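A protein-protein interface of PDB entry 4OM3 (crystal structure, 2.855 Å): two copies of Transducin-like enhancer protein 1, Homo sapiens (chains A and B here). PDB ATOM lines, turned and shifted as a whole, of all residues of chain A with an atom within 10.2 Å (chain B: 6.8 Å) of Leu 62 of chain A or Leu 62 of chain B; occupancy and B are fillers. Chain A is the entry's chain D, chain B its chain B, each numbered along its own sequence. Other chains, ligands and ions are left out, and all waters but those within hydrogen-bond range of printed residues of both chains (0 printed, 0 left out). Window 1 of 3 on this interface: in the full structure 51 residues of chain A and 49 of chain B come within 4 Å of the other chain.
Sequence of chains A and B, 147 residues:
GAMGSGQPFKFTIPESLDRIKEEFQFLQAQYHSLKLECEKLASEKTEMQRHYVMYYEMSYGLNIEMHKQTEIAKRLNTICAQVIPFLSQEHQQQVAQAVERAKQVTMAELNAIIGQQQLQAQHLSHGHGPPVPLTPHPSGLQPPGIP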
ATOM      1  N   MET A  54     -38.629 -22.169  -9.330  1.00  0.00           N
ATOM      2  CA  MET A  54     -37.325 -22.751  -9.039  1.00  0.00           C
ATOM      3  C   MET A  54     -36.815 -23.612 -10.193  1.00  0.00           C
ATOM      4  O   MET A  54     -35.728 -23.369 -10.739  1.00  0.00           O
ATOM      5  CB  MET A  54     -37.412 -23.584  -7.758  1.00  0.00           C
ATOM      6  CG  MET A  54     -36.082 -24.080  -7.229  1.00  0.00           C
ATOM      7  SD  MET A  54     -36.264 -24.855  -5.612  1.00  0.00           S
ATOM      8  CE  MET A  54     -34.551 -25.161  -5.192  1.00  0.00           C
ATOM      9  N   TYR A  55     -37.608 -24.604 -10.581  1.00  0.00           N
ATOM     10  CA  TYR A  55     -37.175 -25.533 -11.619  1.00  0.00           C
ATOM     11  C   TYR A  55     -37.195 -24.956 -13.036  1.00  0.00           C
ATOM     12  O   TYR A  55     -36.436 -25.405 -13.898  1.00  0.00           O
ATOM     13  CB  TYR A  55     -37.930 -26.861 -11.524  1.00  0.00           C
ATOM     14  CG  TYR A  55     -37.401 -27.730 -10.407  1.00  0.00           C
ATOM     15  CD1 TYR A  55     -37.925 -27.642  -9.125  1.00  0.00           C
ATOM     16  CD2 TYR A  55     -36.354 -28.615 -10.628  1.00  0.00           C
ATOM     17  CE1 TYR A  55     -37.434 -28.426  -8.097  1.00  0.00           C
ATOM     18  CE2 TYR A  55     -35.857 -29.403  -9.608  1.00  0.00           C
ATOM     19  CZ  TYR A  55     -36.401 -29.305  -8.345  1.00  0.00           C
ATOM     20  OH  TYR A  55     -35.908 -30.087  -7.327  1.00  0.00           O
ATOM     21  N   TYR A  56     -38.043 -23.957 -13.277  1.00  0.00           N
ATOM     22  CA  TYR A  56     -37.970 -23.231 -14.539  1.00  0.00           C
ATOM     23  C   TYR A  56     -36.616 -22.546 -14.662  1.00  0.00           C
ATOM     24  O   TYR A  56     -35.906 -22.729 -15.654  1.00  0.00           O
ATOM     25  CB  TYR A  56     -39.074 -22.179 -14.668  1.00  0.00           C
ATOM     26  CG  TYR A  56     -38.667 -21.027 -15.568  1.00  0.00           C
ATOM     27  CD1 TYR A  56     -38.599 -21.186 -16.948  1.00  0.00           C
ATOM     28  CD2 TYR A  56     -38.328 -19.788 -15.036  1.00  0.00           C
ATOM     29  CE1 TYR A  56     -38.214 -20.142 -17.771  1.00  0.00           C
ATOM     30  CE2 TYR A  56     -37.941 -18.740 -15.852  1.00  0.00           C
ATOM     31  CZ  TYR A  56     -37.888 -18.921 -17.217  1.00  0.00           C
ATOM     32  OH  TYR A  56     -37.506 -17.879 -18.031  1.00  0.00           O
ATOM     33  N   GLU A  57     -36.269 -21.751 -13.651  1.00  0.00           N
ATOM     34  CA  GLU A  57     -35.013 -21.007 -13.673  1.00  0.00           C
ATOM     35  C   GLU A  57     -33.815 -21.946 -13.785  1.00  0.00           C
ATOM     36  O   GLU A  57     -32.895 -21.714 -14.586  1.00  0.00           O
ATOM     37  CB  GLU A  57     -34.886 -20.117 -12.436  1.00  0.00           C
ATOM     38  CG  GLU A  57     -35.876 -18.963 -12.401  1.00  0.00           C
ATOM     39  CD  GLU A  57     -35.553 -17.949 -11.321  1.00  0.00           C
ATOM     40  OE1 GLU A  57     -36.224 -16.897 -11.271  1.00  0.00           O
ATOM     41  OE2 GLU A  57     -34.625 -18.203 -10.524  1.00  0.00           O
ATOM     42  N   MET A  58     -33.839 -23.012 -12.986  1.00  0.00           N
ATOM     43  CA  MET A  58     -32.801 -24.033 -13.059  1.00  0.00           C
ATOM     44  C   MET A  58     -32.688 -24.574 -14.482  1.00  0.00           C
ATOM     45  O   MET A  58     -31.586 -24.747 -15.005  1.00  0.00           O
ATOM     46  CB  MET A  58     -33.098 -25.174 -12.087  1.00  0.00           C
ATOM     47  CG  MET A  58     -32.126 -26.337 -12.191  1.00  0.00           C
ATOM     48  SD  MET A  58     -32.541 -27.699 -11.088  1.00  0.00           S
ATOM     49  CE  MET A  58     -32.304 -26.925  -9.490  1.00  0.00           C
ATOM     50  N   SER A  59     -33.836 -24.821 -15.106  1.00  0.00           N
ATOM     51  CA  SER A  59     -33.870 -25.305 -16.484  1.00  0.00           C
ATOM     52  C   SER A  59     -33.264 -24.310 -17.478  1.00  0.00           C
ATOM     53  O   SER A  59     -32.617 -24.711 -18.451  1.00  0.00           O
ATOM     54  CB  SER A  59     -35.300 -25.673 -16.891  1.00  0.00           C
ATOM     55  OG  SER A  59     -35.695 -26.898 -16.298  1.00  0.00           O
ATOM     56  N   TYR A  60     -33.469 -23.019 -17.231  1.00  0.00           N
ATOM     57  CA  TYR A  60     -32.884 -21.978 -18.073  1.00  0.00           C
ATOM     58  C   TYR A  60     -31.362 -22.021 -17.966  1.00  0.00           C
ATOM     59  O   TYR A  60     -30.644 -21.963 -18.979  1.00  0.00           O
ATOM     60  CB  TYR A  60     -33.402 -20.598 -17.661  1.00  0.00           C
ATOM     61  CG  TYR A  60     -33.105 -19.501 -18.662  1.00  0.00           C
ATOM     62  CD1 TYR A  60     -33.599 -19.570 -19.956  1.00  0.00           C
ATOM     63  CD2 TYR A  60     -32.347 -18.392 -18.311  1.00  0.00           C
ATOM     64  CE1 TYR A  60     -33.338 -18.575 -20.877  1.00  0.00           C
ATOM     65  CE2 TYR A  60     -32.081 -17.386 -19.228  1.00  0.00           C
ATOM     66  CZ  TYR A  60     -32.582 -17.485 -20.511  1.00  0.00           C
ATOM     67  OH  TYR A  60     -32.324 -16.494 -21.431  1.00  0.00           O
ATOM     68  N   GLY A  61     -30.879 -22.133 -16.731  1.00  0.00           N
ATOM     69  CA  GLY A  61     -29.451 -22.224 -16.478  1.00  0.00           C
ATOM     70  C   GLY A  61     -28.812 -23.420 -17.156  1.00  0.00           C
ATOM     71  O   GLY A  61     -27.844 -23.288 -17.923  1.00  0.00           O
ATOM     72  N   LEU A  62     -29.363 -24.599 -16.877  1.00  0.00           N
ATOM     73  CA  LEU A  62     -28.889 -25.830 -17.501  1.00  0.00           C
ATOM     74  C   LEU A  62     -28.925 -25.741 -19.020  1.00  0.00           C
ATOM     75  O   LEU A  62     -28.095 -26.340 -19.696  1.00  0.00           O
ATOM     76  CB  LEU A  62     -29.739 -27.013 -17.057  1.00  0.00           C
ATOM     77  CG  LEU A  62     -29.675 -27.347 -15.575  1.00  0.00           C
ATOM     78  CD1 LEU A  62     -30.626 -28.482 -15.265  1.00  0.00           C
ATOM     79  CD2 LEU A  62     -28.253 -27.703 -15.184  1.00  0.00           C
ATOM     80  N   ASN A  63     -29.902 -25.000 -19.546  1.00  0.00           N
ATOM     81  CA  ASN A  63     -30.061 -24.823 -20.984  1.00  0.00           C
ATOM     82  C   ASN A  63     -28.847 -24.085 -21.518  1.00  0.00           C
ATOM     83  O   ASN A  63     -28.147 -24.563 -22.421  1.00  0.00           O
ATOM     84  CB  ASN A  63     -31.365 -24.067 -21.295  1.00  0.00           C
ATOM     85  CG  ASN A  63     -31.613 -23.919 -22.783  1.00  0.00           C
ATOM     86  OD1 ASN A  63     -31.176 -24.747 -23.565  1.00  0.00           O
ATOM     87  ND2 ASN A  63     -32.316 -22.872 -23.175  1.00  0.00           N
ATOM     88  N   ILE A  64     -28.590 -22.931 -20.914  1.00  0.00           N
ATOM     89  CA  ILE A  64     -27.469 -22.096 -21.306  1.00  0.00           C
ATOM     90  C   ILE A  64     -26.160 -22.879 -21.272  1.00  0.00           C
ATOM     91  O   ILE A  64     -25.436 -22.945 -22.277  1.00  0.00           O
ATOM     92  CB  ILE A  64     -27.376 -20.857 -20.397  1.00  0.00           C
ATOM     93  CG1 ILE A  64     -28.592 -19.954 -20.624  1.00  0.00           C
ATOM     94  CG2 ILE A  64     -26.075 -20.098 -20.646  1.00  0.00           C
ATOM     95  CD1 ILE A  64     -28.644 -18.762 -19.702  1.00  0.00           C
ATOM     96  N   GLU A  65     -25.870 -23.481 -20.121  1.00  0.00           N
ATOM     97  CA  GLU A  65     -24.638 -24.247 -19.957  1.00  0.00           C
ATOM     98  C   GLU A  65     -24.505 -25.407 -20.948  1.00  0.00           C
ATOM     99  O   GLU A  65     -23.435 -25.603 -21.533  1.00  0.00           O
ATOM    100  CB  GLU A  65     -24.488 -24.741 -18.517  1.00  0.00           C
ATOM    101  CG  GLU A  65     -23.495 -23.932 -17.697  1.00  0.00           C
ATOM    102  CD  GLU A  65     -22.168 -23.735 -18.413  1.00  0.00           C
ATOM    103  OE1 GLU A  65     -21.799 -22.571 -18.678  1.00  0.00           O
ATOM    104  OE2 GLU A  65     -21.489 -24.743 -18.711  1.00  0.00           O
ATOM    105  N   MET A  66     -25.582 -26.167 -21.137  1.00  0.00           N
ATOM    106  CA  MET A  66     -25.581 -27.261 -22.107  1.00  0.00           C
ATOM    107  C   MET A  66     -25.250 -26.777 -23.510  1.00  0.00           C
ATOM    108  O   MET A  66     -24.410 -27.364 -24.190  1.00  0.00           O
ATOM    109  CB  MET A  66     -26.920 -28.019 -22.109  1.00  0.00           C
ATOM    110  CG  MET A  66     -27.001 -29.117 -23.181  1.00  0.00           C
ATOM    111  SD  MET A  66     -28.499 -30.111 -23.248  1.00  0.00           S
ATOM    112  CE  MET A  66     -29.689 -28.977 -23.933  1.00  0.00           C
ATOM    113  N   HIS A  67     -25.904 -25.705 -23.945  1.00  0.00           N
ATOM    114  CA  HIS A  67     -25.707 -25.247 -25.310  1.00  0.00           C
ATOM    115  C   HIS A  67     -24.287 -24.731 -25.472  1.00  0.00           C
ATOM    116  O   HIS A  67     -23.662 -24.900 -26.523  1.00  0.00           O
ATOM    117  CB  HIS A  67     -26.743 -24.191 -25.698  1.00  0.00           C
ATOM    118  CG  HIS A  67     -28.025 -24.768 -26.198  1.00  0.00           C
ATOM    119  ND1 HIS A  67     -29.180 -24.790 -25.449  1.00  0.00           N
ATOM    120  CD2 HIS A  67     -28.332 -25.354 -27.380  1.00  0.00           C
ATOM    121  CE1 HIS A  67     -30.147 -25.359 -26.147  1.00  0.00           C
ATOM    122  NE2 HIS A  67     -29.655 -25.710 -27.322  1.00  0.00           N
ATOM    123  N   LYS A  68     -23.782 -24.116 -24.409  1.00  0.00           N
ATOM    124  CA  LYS A  68     -22.402 -23.659 -24.374  1.00  0.00           C
ATOM    125  C   LYS A  68     -21.425 -24.810 -24.595  1.00  0.00           C
ATOM    126  O   LYS A  68     -20.654 -24.799 -25.558  1.00  0.00           O
ATOM    127  CB  LYS A  68     -22.105 -22.978 -23.039  1.00  0.00           C
ATOM    128  CG  LYS A  68     -20.665 -22.558 -22.884  1.00  0.00           C
ATOM    129  CD  LYS A  68     -20.466 -21.721 -21.641  1.00  0.00           C
ATOM    130  CE  LYS A  68     -19.019 -21.296 -21.517  1.00  0.00           C
ATOM    131  NZ  LYS A  68     -18.807 -20.359 -20.386  1.00  0.00           N
ATOM    132  N   GLN A  69     -21.464 -25.803 -23.709  1.00  0.00           N
ATOM    133  CA  GLN A  69     -20.538 -26.931 -23.809  1.00  0.00           C
ATOM    134  C   GLN A  69     -20.698 -27.690 -25.123  1.00  0.00           C
ATOM    135  O   GLN A  69     -19.732 -28.243 -25.652  1.00  0.00           O
ATOM    136  CB  GLN A  69     -20.699 -27.881 -22.621  1.00  0.00           C
ATOM    137  CG  GLN A  69     -20.548 -27.212 -21.266  1.00  0.00           C
ATOM    138  CD  GLN A  69     -19.226 -26.485 -21.107  1.00  0.00           C
ATOM    139  OE1 GLN A  69     -18.205 -26.891 -21.664  1.00  0.00           O
ATOM    140  NE2 GLN A  69     -19.239 -25.399 -20.343  1.00  0.00           N
ATOM    141  N   THR A  70     -21.919 -27.706 -25.645  1.00  0.00           N
ATOM    142  CA  THR A  70     -22.189 -28.314 -26.941  1.00  0.00           C
ATOM    143  C   THR A  70     -21.420 -27.576 -28.031  1.00  0.00           C
ATOM    144  O   THR A  70     -20.745 -28.193 -28.862  1.00  0.00           O
ATOM    145  CB  THR A  70     -23.690 -28.282 -27.273  1.00  0.00           C
ATOM    146  OG1 THR A  70     -24.441 -28.780 -26.158  1.00  0.00           O
ATOM    147  CG2 THR A  70     -23.980 -29.131 -28.500  1.00  0.00           C
ATOM    148  N   LEU A 110     -21.506 -41.709 -17.577  1.00  0.00           N
ATOM    149  CA  LEU A 110     -22.350 -40.523 -17.513  1.00  0.00           C
ATOM    150  C   LEU A 110     -23.042 -40.484 -16.156  1.00  0.00           C
ATOM    151  O   LEU A 110     -23.119 -39.437 -15.511  1.00  0.00           O
ATOM    152  CB  LEU A 110     -23.379 -40.534 -18.643  1.00  0.00           C
ATOM    153  CG  LEU A 110     -24.123 -39.234 -18.946  1.00  0.00           C
ATOM    154  CD1 LEU A 110     -23.154 -38.067 -19.025  1.00  0.00           C
ATOM    155  CD2 LEU A 110     -24.891 -39.375 -20.249  1.00  0.00           C
ATOM    156  N   ILE A 114     -22.356 -37.544 -13.417  1.00  0.00           N
ATOM    157  CA  ILE A 114     -23.561 -36.883 -12.920  1.00  0.00           C
ATOM    158  C   ILE A 114     -23.739 -37.105 -11.418  1.00  0.00           C
ATOM    159  O   ILE A 114     -23.868 -36.147 -10.656  1.00  0.00           O
ATOM    160  CB  ILE A 114     -24.822 -37.370 -13.653  1.00  0.00           C
ATOM    161  CG1 ILE A 114     -24.847 -36.841 -15.085  1.00  0.00           C
ATOM    162  CG2 ILE A 114     -26.074 -36.918 -12.919  1.00  0.00           C
ATOM    163  CD1 ILE A 114     -25.989 -37.387 -15.901  1.00  0.00           C
ATOM    164  N   GLN A 117     -20.739 -35.128  -9.552  1.00  0.00           N
ATOM    165  CA  GLN A 117     -20.981 -33.676  -9.536  1.00  0.00           C
ATOM    166  C   GLN A 117     -22.169 -33.308  -8.640  1.00  0.00           C
ATOM    167  O   GLN A 117     -22.178 -32.260  -7.987  1.00  0.00           O
ATOM    168  CB  GLN A 117     -21.205 -33.146 -10.956  1.00  0.00           C
ATOM    169  CG  GLN A 117     -21.414 -31.643 -11.038  1.00  0.00           C
ATOM    170  CD  GLN A 117     -20.149 -30.856 -10.768  1.00  0.00           C
ATOM    171  OE1 GLN A 117     -19.050 -31.282 -11.123  1.00  0.00           O
ATOM    172  NE2 GLN A 117     -20.296 -29.700 -10.132  1.00  0.00           N
ATOM    173  N   ALA A 121     -22.032 -30.939  -5.477  1.00  0.00           N
ATOM    174  CA  ALA A 121     -22.861 -29.745  -5.365  1.00  0.00           C
ATOM    175  C   ALA A 121     -23.736 -29.796  -4.117  1.00  0.00           C
ATOM    176  O   ALA A 121     -24.962 -29.739  -4.204  1.00  0.00           O
ATOM    177  CB  ALA A 121     -23.718 -29.575  -6.609  1.00  0.00           C
ATOM    178  N   GLY A 127     -31.603 -29.663  -5.617  1.00  0.00           N
ATOM    179  CA  GLY A 127     -32.510 -30.268  -6.574  1.00  0.00           C
ATOM    180  C   GLY A 127     -31.747 -31.051  -7.621  1.00  0.00           C
ATOM    181  O   GLY A 127     -30.747 -31.688  -7.299  1.00  0.00           O
ATOM    182  N   HIS A 128     -32.208 -30.985  -8.869  1.00  0.00           N
ATOM    183  CA  HIS A 128     -31.601 -31.711  -9.995  1.00  0.00           C
ATOM    184  C   HIS A 128     -31.148 -33.137  -9.661  1.00  0.00           C
ATOM    185  O   HIS A 128     -29.961 -33.454  -9.728  1.00  0.00           O
ATOM    186  CB  HIS A 128     -30.422 -30.915 -10.534  1.00  0.00           C
ATOM    187  N   GLY A 129     -32.105 -33.983  -9.296  1.00  0.00           N
ATOM    188  CA  GLY A 129     -31.820 -35.372  -9.001  1.00  0.00           C
ATOM    189  C   GLY A 129     -32.108 -36.267 -10.189  1.00  0.00           C
ATOM    190  O   GLY A 129     -32.954 -35.939 -11.019  1.00  0.00           O
ATOM    191  N   PRO A 130     -31.389 -37.395 -10.292  1.00  0.00           N
ATOM    192  CA  PRO A 130     -31.560 -38.360 -11.390  1.00  0.00           C
ATOM    193  C   PRO A 130     -32.924 -39.068 -11.526  1.00  0.00           C
ATOM    194  O   PRO A 130     -33.221 -39.544 -12.624  1.00  0.00           O
ATOM    195  CB  PRO A 130     -30.473 -39.418 -11.278  1.00  0.00           C
ATOM    196  N   TYR B  55     -40.732 -28.964 -15.912  1.00  0.00           N
ATOM    197  CA  TYR B  55     -39.408 -28.393 -15.702  1.00  0.00           C
ATOM    198  C   TYR B  55     -38.527 -29.272 -14.819  1.00  0.00           C
ATOM    199  O   TYR B  55     -37.311 -29.105 -14.794  1.00  0.00           O
ATOM    200  CB  TYR B  55     -39.506 -26.969 -15.144  1.00  0.00           C
ATOM    201  CG  TYR B  55     -40.095 -25.987 -16.130  1.00  0.00           C
ATOM    202  CD1 TYR B  55     -39.394 -25.622 -17.272  1.00  0.00           C
ATOM    203  CD2 TYR B  55     -41.344 -25.420 -15.921  1.00  0.00           C
ATOM    204  CE1 TYR B  55     -39.922 -24.726 -18.180  1.00  0.00           C
ATOM    205  CE2 TYR B  55     -41.882 -24.522 -16.823  1.00  0.00           C
ATOM    206  CZ  TYR B  55     -41.167 -24.177 -17.950  1.00  0.00           C
ATOM    207  OH  TYR B  55     -41.703 -23.282 -18.848  1.00  0.00           O
ATOM    208  N   GLU B  57     -38.467 -32.804 -15.125  1.00  0.00           N
ATOM    209  CA  GLU B  57     -37.882 -33.756 -16.079  1.00  0.00           C
ATOM    210  C   GLU B  57     -36.960 -33.050 -17.071  1.00  0.00           C
ATOM    211  O   GLU B  57     -35.934 -33.602 -17.499  1.00  0.00           O
ATOM    212  CB  GLU B  57     -38.955 -34.574 -16.817  1.00  0.00           C
ATOM    213  CG  GLU B  57     -39.620 -33.883 -18.004  1.00  0.00           C
ATOM    214  CD  GLU B  57     -40.408 -34.853 -18.873  1.00  0.00           C
ATOM    215  OE1 GLU B  57     -40.467 -36.055 -18.530  1.00  0.00           O
ATOM    216  OE2 GLU B  57     -40.966 -34.416 -19.903  1.00  0.00           O
ATOM    217  N   MET B  58     -37.325 -31.820 -17.418  1.00  0.00           N
ATOM    218  CA  MET B  58     -36.505 -31.015 -18.305  1.00  0.00           C
ATOM    219  C   MET B  58     -35.171 -30.756 -17.627  1.00  0.00           C
ATOM    220  O   MET B  58     -34.126 -30.945 -18.236  1.00  0.00           O
ATOM    221  CB  MET B  58     -37.204 -29.699 -18.646  1.00  0.00           C
ATOM    222  CG  MET B  58     -36.775 -29.108 -19.976  1.00  0.00           C
ATOM    223  SD  MET B  58     -37.529 -27.503 -20.303  1.00  0.00           S
ATOM    224  CE  MET B  58     -39.261 -27.877 -20.047  1.00  0.00           C
ATOM    225  N   SER B  59     -35.214 -30.353 -16.358  1.00  0.00           N
ATOM    226  CA  SER B  59     -34.003 -30.116 -15.576  1.00  0.00           C
ATOM    227  C   SER B  59     -33.115 -31.354 -15.595  1.00  0.00           C
ATOM    228  O   SER B  59     -31.907 -31.265 -15.815  1.00  0.00           O
ATOM    229  CB  SER B  59     -34.358 -29.755 -14.131  1.00  0.00           C
ATOM    230  OG  SER B  59     -33.291 -29.081 -13.487  1.00  0.00           O
ATOM    231  N   TYR B  60     -33.734 -32.509 -15.377  1.00  0.00           N
ATOM    232  CA  TYR B  60     -33.036 -33.789 -15.424  1.00  0.00           C
ATOM    233  C   TYR B  60     -32.270 -33.993 -16.737  1.00  0.00           C
ATOM    234  O   TYR B  60     -31.031 -34.125 -16.744  1.00  0.00           O
ATOM    235  CB  TYR B  60     -34.042 -34.920 -15.212  1.00  0.00           C
ATOM    236  CG  TYR B  60     -33.470 -36.307 -15.370  1.00  0.00           C
ATOM    237  CD1 TYR B  60     -32.350 -36.704 -14.654  1.00  0.00           C
ATOM    238  CD2 TYR B  60     -34.068 -37.230 -16.219  1.00  0.00           C
ATOM    239  CE1 TYR B  60     -31.827 -37.972 -14.793  1.00  0.00           C
ATOM    240  CE2 TYR B  60     -33.558 -38.504 -16.362  1.00  0.00           C
ATOM    241  CZ  TYR B  60     -32.439 -38.871 -15.644  1.00  0.00           C
ATOM    242  OH  TYR B  60     -31.926 -40.141 -15.784  1.00  0.00           O
ATOM    243  N   GLY B  61     -33.012 -34.012 -17.843  1.00  0.00           N
ATOM    244  CA  GLY B  61     -32.416 -34.206 -19.155  1.00  0.00           C
ATOM    245  C   GLY B  61     -31.330 -33.195 -19.491  1.00  0.00           C
ATOM    246  O   GLY B  61     -30.239 -33.563 -19.942  1.00  0.00           O
ATOM    247  N   LEU B  62     -31.635 -31.919 -19.264  1.00  0.00           N
ATOM    248  CA  LEU B  62     -30.685 -30.832 -19.492  1.00  0.00           C
ATOM    249  C   LEU B  62     -29.395 -31.073 -18.718  1.00  0.00           C
ATOM    250  O   LEU B  62     -28.307 -30.842 -19.238  1.00  0.00           O
ATOM    251  CB  LEU B  62     -31.274 -29.480 -19.068  1.00  0.00           C
ATOM    252  CG  LEU B  62     -32.483 -28.851 -19.772  1.00  0.00           C
ATOM    253  CD1 LEU B  62     -33.250 -27.998 -18.771  1.00  0.00           C
ATOM    254  CD2 LEU B  62     -32.118 -28.020 -20.994  1.00  0.00           C
ATOM    255  N   ASN B  63     -29.526 -31.527 -17.472  1.00  0.00           N
ATOM    256  CA  ASN B  63     -28.367 -31.838 -16.635  1.00  0.00           C
ATOM    257  C   ASN B  63     -27.516 -32.938 -17.262  1.00  0.00           C
ATOM    258  O   ASN B  63     -26.289 -32.803 -17.394  1.00  0.00           O
ATOM    259  CB  ASN B  63     -28.816 -32.259 -15.232  1.00  0.00           C
ATOM    260  CG  ASN B  63     -27.667 -32.310 -14.236  1.00  0.00           C
ATOM    261  OD1 ASN B  63     -26.703 -31.551 -14.343  1.00  0.00           O
ATOM    262  ND2 ASN B  63     -27.768 -33.206 -13.260  1.00  0.00           N
ATOM    263  N   ILE B  64     -28.183 -34.024 -17.652  1.00  0.00           N
ATOM    264  CA  ILE B  64     -27.497 -35.146 -18.287  1.00  0.00           C
ATOM    265  C   ILE B  64     -26.704 -34.720 -19.523  1.00  0.00           C
ATOM    266  O   ILE B  64     -25.498 -34.992 -19.632  1.00  0.00           O
ATOM    267  CB  ILE B  64     -28.484 -36.261 -18.680  1.00  0.00           C
ATOM    268  CG1 ILE B  64     -29.189 -36.810 -17.438  1.00  0.00           C
ATOM    269  CG2 ILE B  64     -27.765 -37.374 -19.419  1.00  0.00           C
ATOM    270  CD1 ILE B  64     -29.882 -38.129 -17.673  1.00  0.00           C
ATOM    271  N   GLU B  65     -27.376 -34.041 -20.447  1.00  0.00           N
ATOM    272  CA  GLU B  65     -26.730 -33.638 -21.692  1.00  0.00           C
ATOM    273  C   GLU B  65     -25.626 -32.611 -21.444  1.00  0.00           C
ATOM    274  O   GLU B  65     -24.603 -32.605 -22.137  1.00  0.00           O
ATOM    275  CB  GLU B  65     -27.761 -33.106 -22.688  1.00  0.00           C
ATOM    276  CG  GLU B  65     -27.291 -33.120 -24.137  1.00  0.00           C
ATOM    277  CD  GLU B  65     -27.133 -34.519 -24.695  1.00  0.00           C
ATOM    278  OE1 GLU B  65     -27.637 -35.477 -24.070  1.00  0.00           O
ATOM    279  OE2 GLU B  65     -26.504 -34.661 -25.765  1.00  0.00           O
ATOM    280  N   MET B  66     -25.835 -31.757 -20.445  1.00  0.00           N
ATOM    281  CA  MET B  66     -24.836 -30.769 -20.056  1.00  0.00           C
ATOM    282  C   MET B  66     -23.542 -31.448 -19.637  1.00  0.00           C
ATOM    283  O   MET B  66     -22.465 -31.108 -20.130  1.00  0.00           O
ATOM    284  CB  MET B  66     -25.349 -29.907 -18.903  1.00  0.00           C
ATOM    285  CG  MET B  66     -24.352 -28.868 -18.421  1.00  0.00           C
ATOM    286  SD  MET B  66     -24.970 -27.916 -17.021  1.00  0.00           S
ATOM    287  CE  MET B  66     -24.862 -29.126 -15.707  1.00  0.00           C
ATOM    288  N   HIS B  67     -23.652 -32.410 -18.726  1.00  0.00           N
ATOM    289  CA  HIS B  67     -22.464 -33.117 -18.256  1.00  0.00           C
ATOM    290  C   HIS B  67     -21.809 -33.966 -19.347  1.00  0.00           C
ATOM    291  O   HIS B  67     -20.578 -34.053 -19.422  1.00  0.00           O
ATOM    292  CB  HIS B  67     -22.780 -33.945 -17.011  1.00  0.00           C
ATOM    293  CG  HIS B  67     -22.817 -33.138 -15.751  1.00  0.00           C
ATOM    294  ND1 HIS B  67     -23.785 -33.305 -14.784  1.00  0.00           N
ATOM    295  CD2 HIS B  67     -22.003 -32.153 -15.303  1.00  0.00           C
ATOM    296  CE1 HIS B  67     -23.564 -32.458 -13.794  1.00  0.00           C
ATOM    297  NE2 HIS B  67     -22.490 -31.747 -14.085  1.00  0.00           N
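SD of Met 58 of chain A lies within hydrogen-bond range of OG of Ser 59 of chain B, at 2.9 Å. The side-chain hydroxyl (OG) of Ser 59 of chain A is in hydrogen-bond range of the backbone carbonyl oxygen (O) of Tyr 55 of chain B, 3.1 Å away. OG of Ser 59 of chain A is in hydrogen-bond range of N of Ser 59 of chain B (3.5 Å). The side-chain hydroxyl (OH) of Tyr 60 of chain B sits close to the backbone carbonyl oxygen (O) of Pro 130 of chain A (3.5 Å).
Tyr 55 of chain A touches its own counterpart, Tyr 55 of chain B. Met 58 of chain A touches Ser 59 of chain B, and with the chains exchanged Ser 59 of chain A touches Met 58 of chain B. Ser 59 of chain B touches its own counterpart, Ser 59 of chain A. Leu 62 of chain B touches its own counterpart, Leu 62 of chain A. Of the 22 pairs that touch across the chains among the printed residues, 14 have their exchanged pair printed and touching as well.
Of the 12 printed residues of chain B, 10 touch a printed residue of chain A. Hydrophobic or aromatic side chains of chain B that line the printed part of chain A: Tyr 55, Met 58, Tyr 60, Leu 62, Ile 64, Met 66 and His 67. Along chain B the printed residues that touch a printed residue of chain A span positions 55 to 67. Printed residues of chain A that touch a printed residue of chain B: Tyr 55, Tyr 56, Met 58, Ser 59, Leu 62, Asn 63, Glu 65, Met 66, Leu 110, Ile 114, Gln 117, Gly 129 and Pro 130. Hydrophobic or aromatic side chains of chain A within 4 Å of the printed part of chain B: Tyr 55, Tyr 56, Met 58, Leu 62, Met 66, Leu 110 and Ile 114. Among the printed residues, no Asp or Glu carboxylate lies within 4 Å of a Lys or Arg side-chain nitrogen of the other chain.
The side-chain amide nitrogen (NE2) of Gln 69 of chain A sits at hydrogen-bond distance from the side-chain carboxylate (OE2) of Glu 65 of chain A (2.9 Å). The backbone carbonyl oxygen (O) of Met 66 of chain A lies within hydrogen-bond range of the side-chain hydroxyl (OG1) of Thr 70 of chain A (2.4 Å). The side-chain amide oxygen (OD1) of Asn 63 of chain A is in hydrogen-bond range of a ring nitrogen (ND1) of His 67 of chain A (2.7 Å).
Among the printed residues, merely in contact across the chains: Leu 62 of chain A with Ser 59 of chain B, Met 66 of chain A with Glu 65 of chain B, Gln 117 of chain A with His 67 of chain B, Ser 59 of chain A with Leu 62 of chain B, Leu 62 of chain A with Leu 62 of chain B, Glu 65 of chain A with Met 66 of chain B, Ile 114 of chain A with Ile 64 of chain B, Leu 110 of chain A with Ile 64 of chain B, Tyr 55 of chain A with Tyr 55 of chain B, Ile 114 of chain A with His 67 of chain B, Leu 62 of chain A with Met 66 of chain B, Gly 129 of chain A with Tyr 60 of chain B, Asn 63 of chain A with Leu 62 of chain B, Tyr 56 of chain A with Tyr 55 of chain B, Leu 62 of chain A with Asn 63 of chain B, Met 66 of chain A with Leu 62 of chain B, Ser 59 of chain A with Met 58 of chain B and Met 66 of chain A with Met 66 of chain B.
Leu 62 of chain A touches just these residues of chain B: Ser 59 (3.1 Å), Leu 62 (3.5 Å), Asn 63 (3.9 Å) and Met 66 (3.7 Å). Of chain A, only Ser 59 (3.4 Å), Leu 62 (3.5 Å), Asn 63 (3.8 Å) and Met 66 (3.9 Å) come within 4 Å of Leu 62 of chain B. Of chain A, only Ser 59 comes within 4 Å of Met 58 of chain B. No residue of chain A comes within 4 Å of Gly 61 of chain B. Of the printed residues of chain B, Leu 110 of chain A touches Ile 64 (3.6 Å). Of the printed residues of chain B, Gly 129 of chain A touches Tyr 60 (3.8 Å). The nearest printed residue of chain B that does not touch Ile 114 of chain A is Asn 63 of chain B (4.1 Å).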
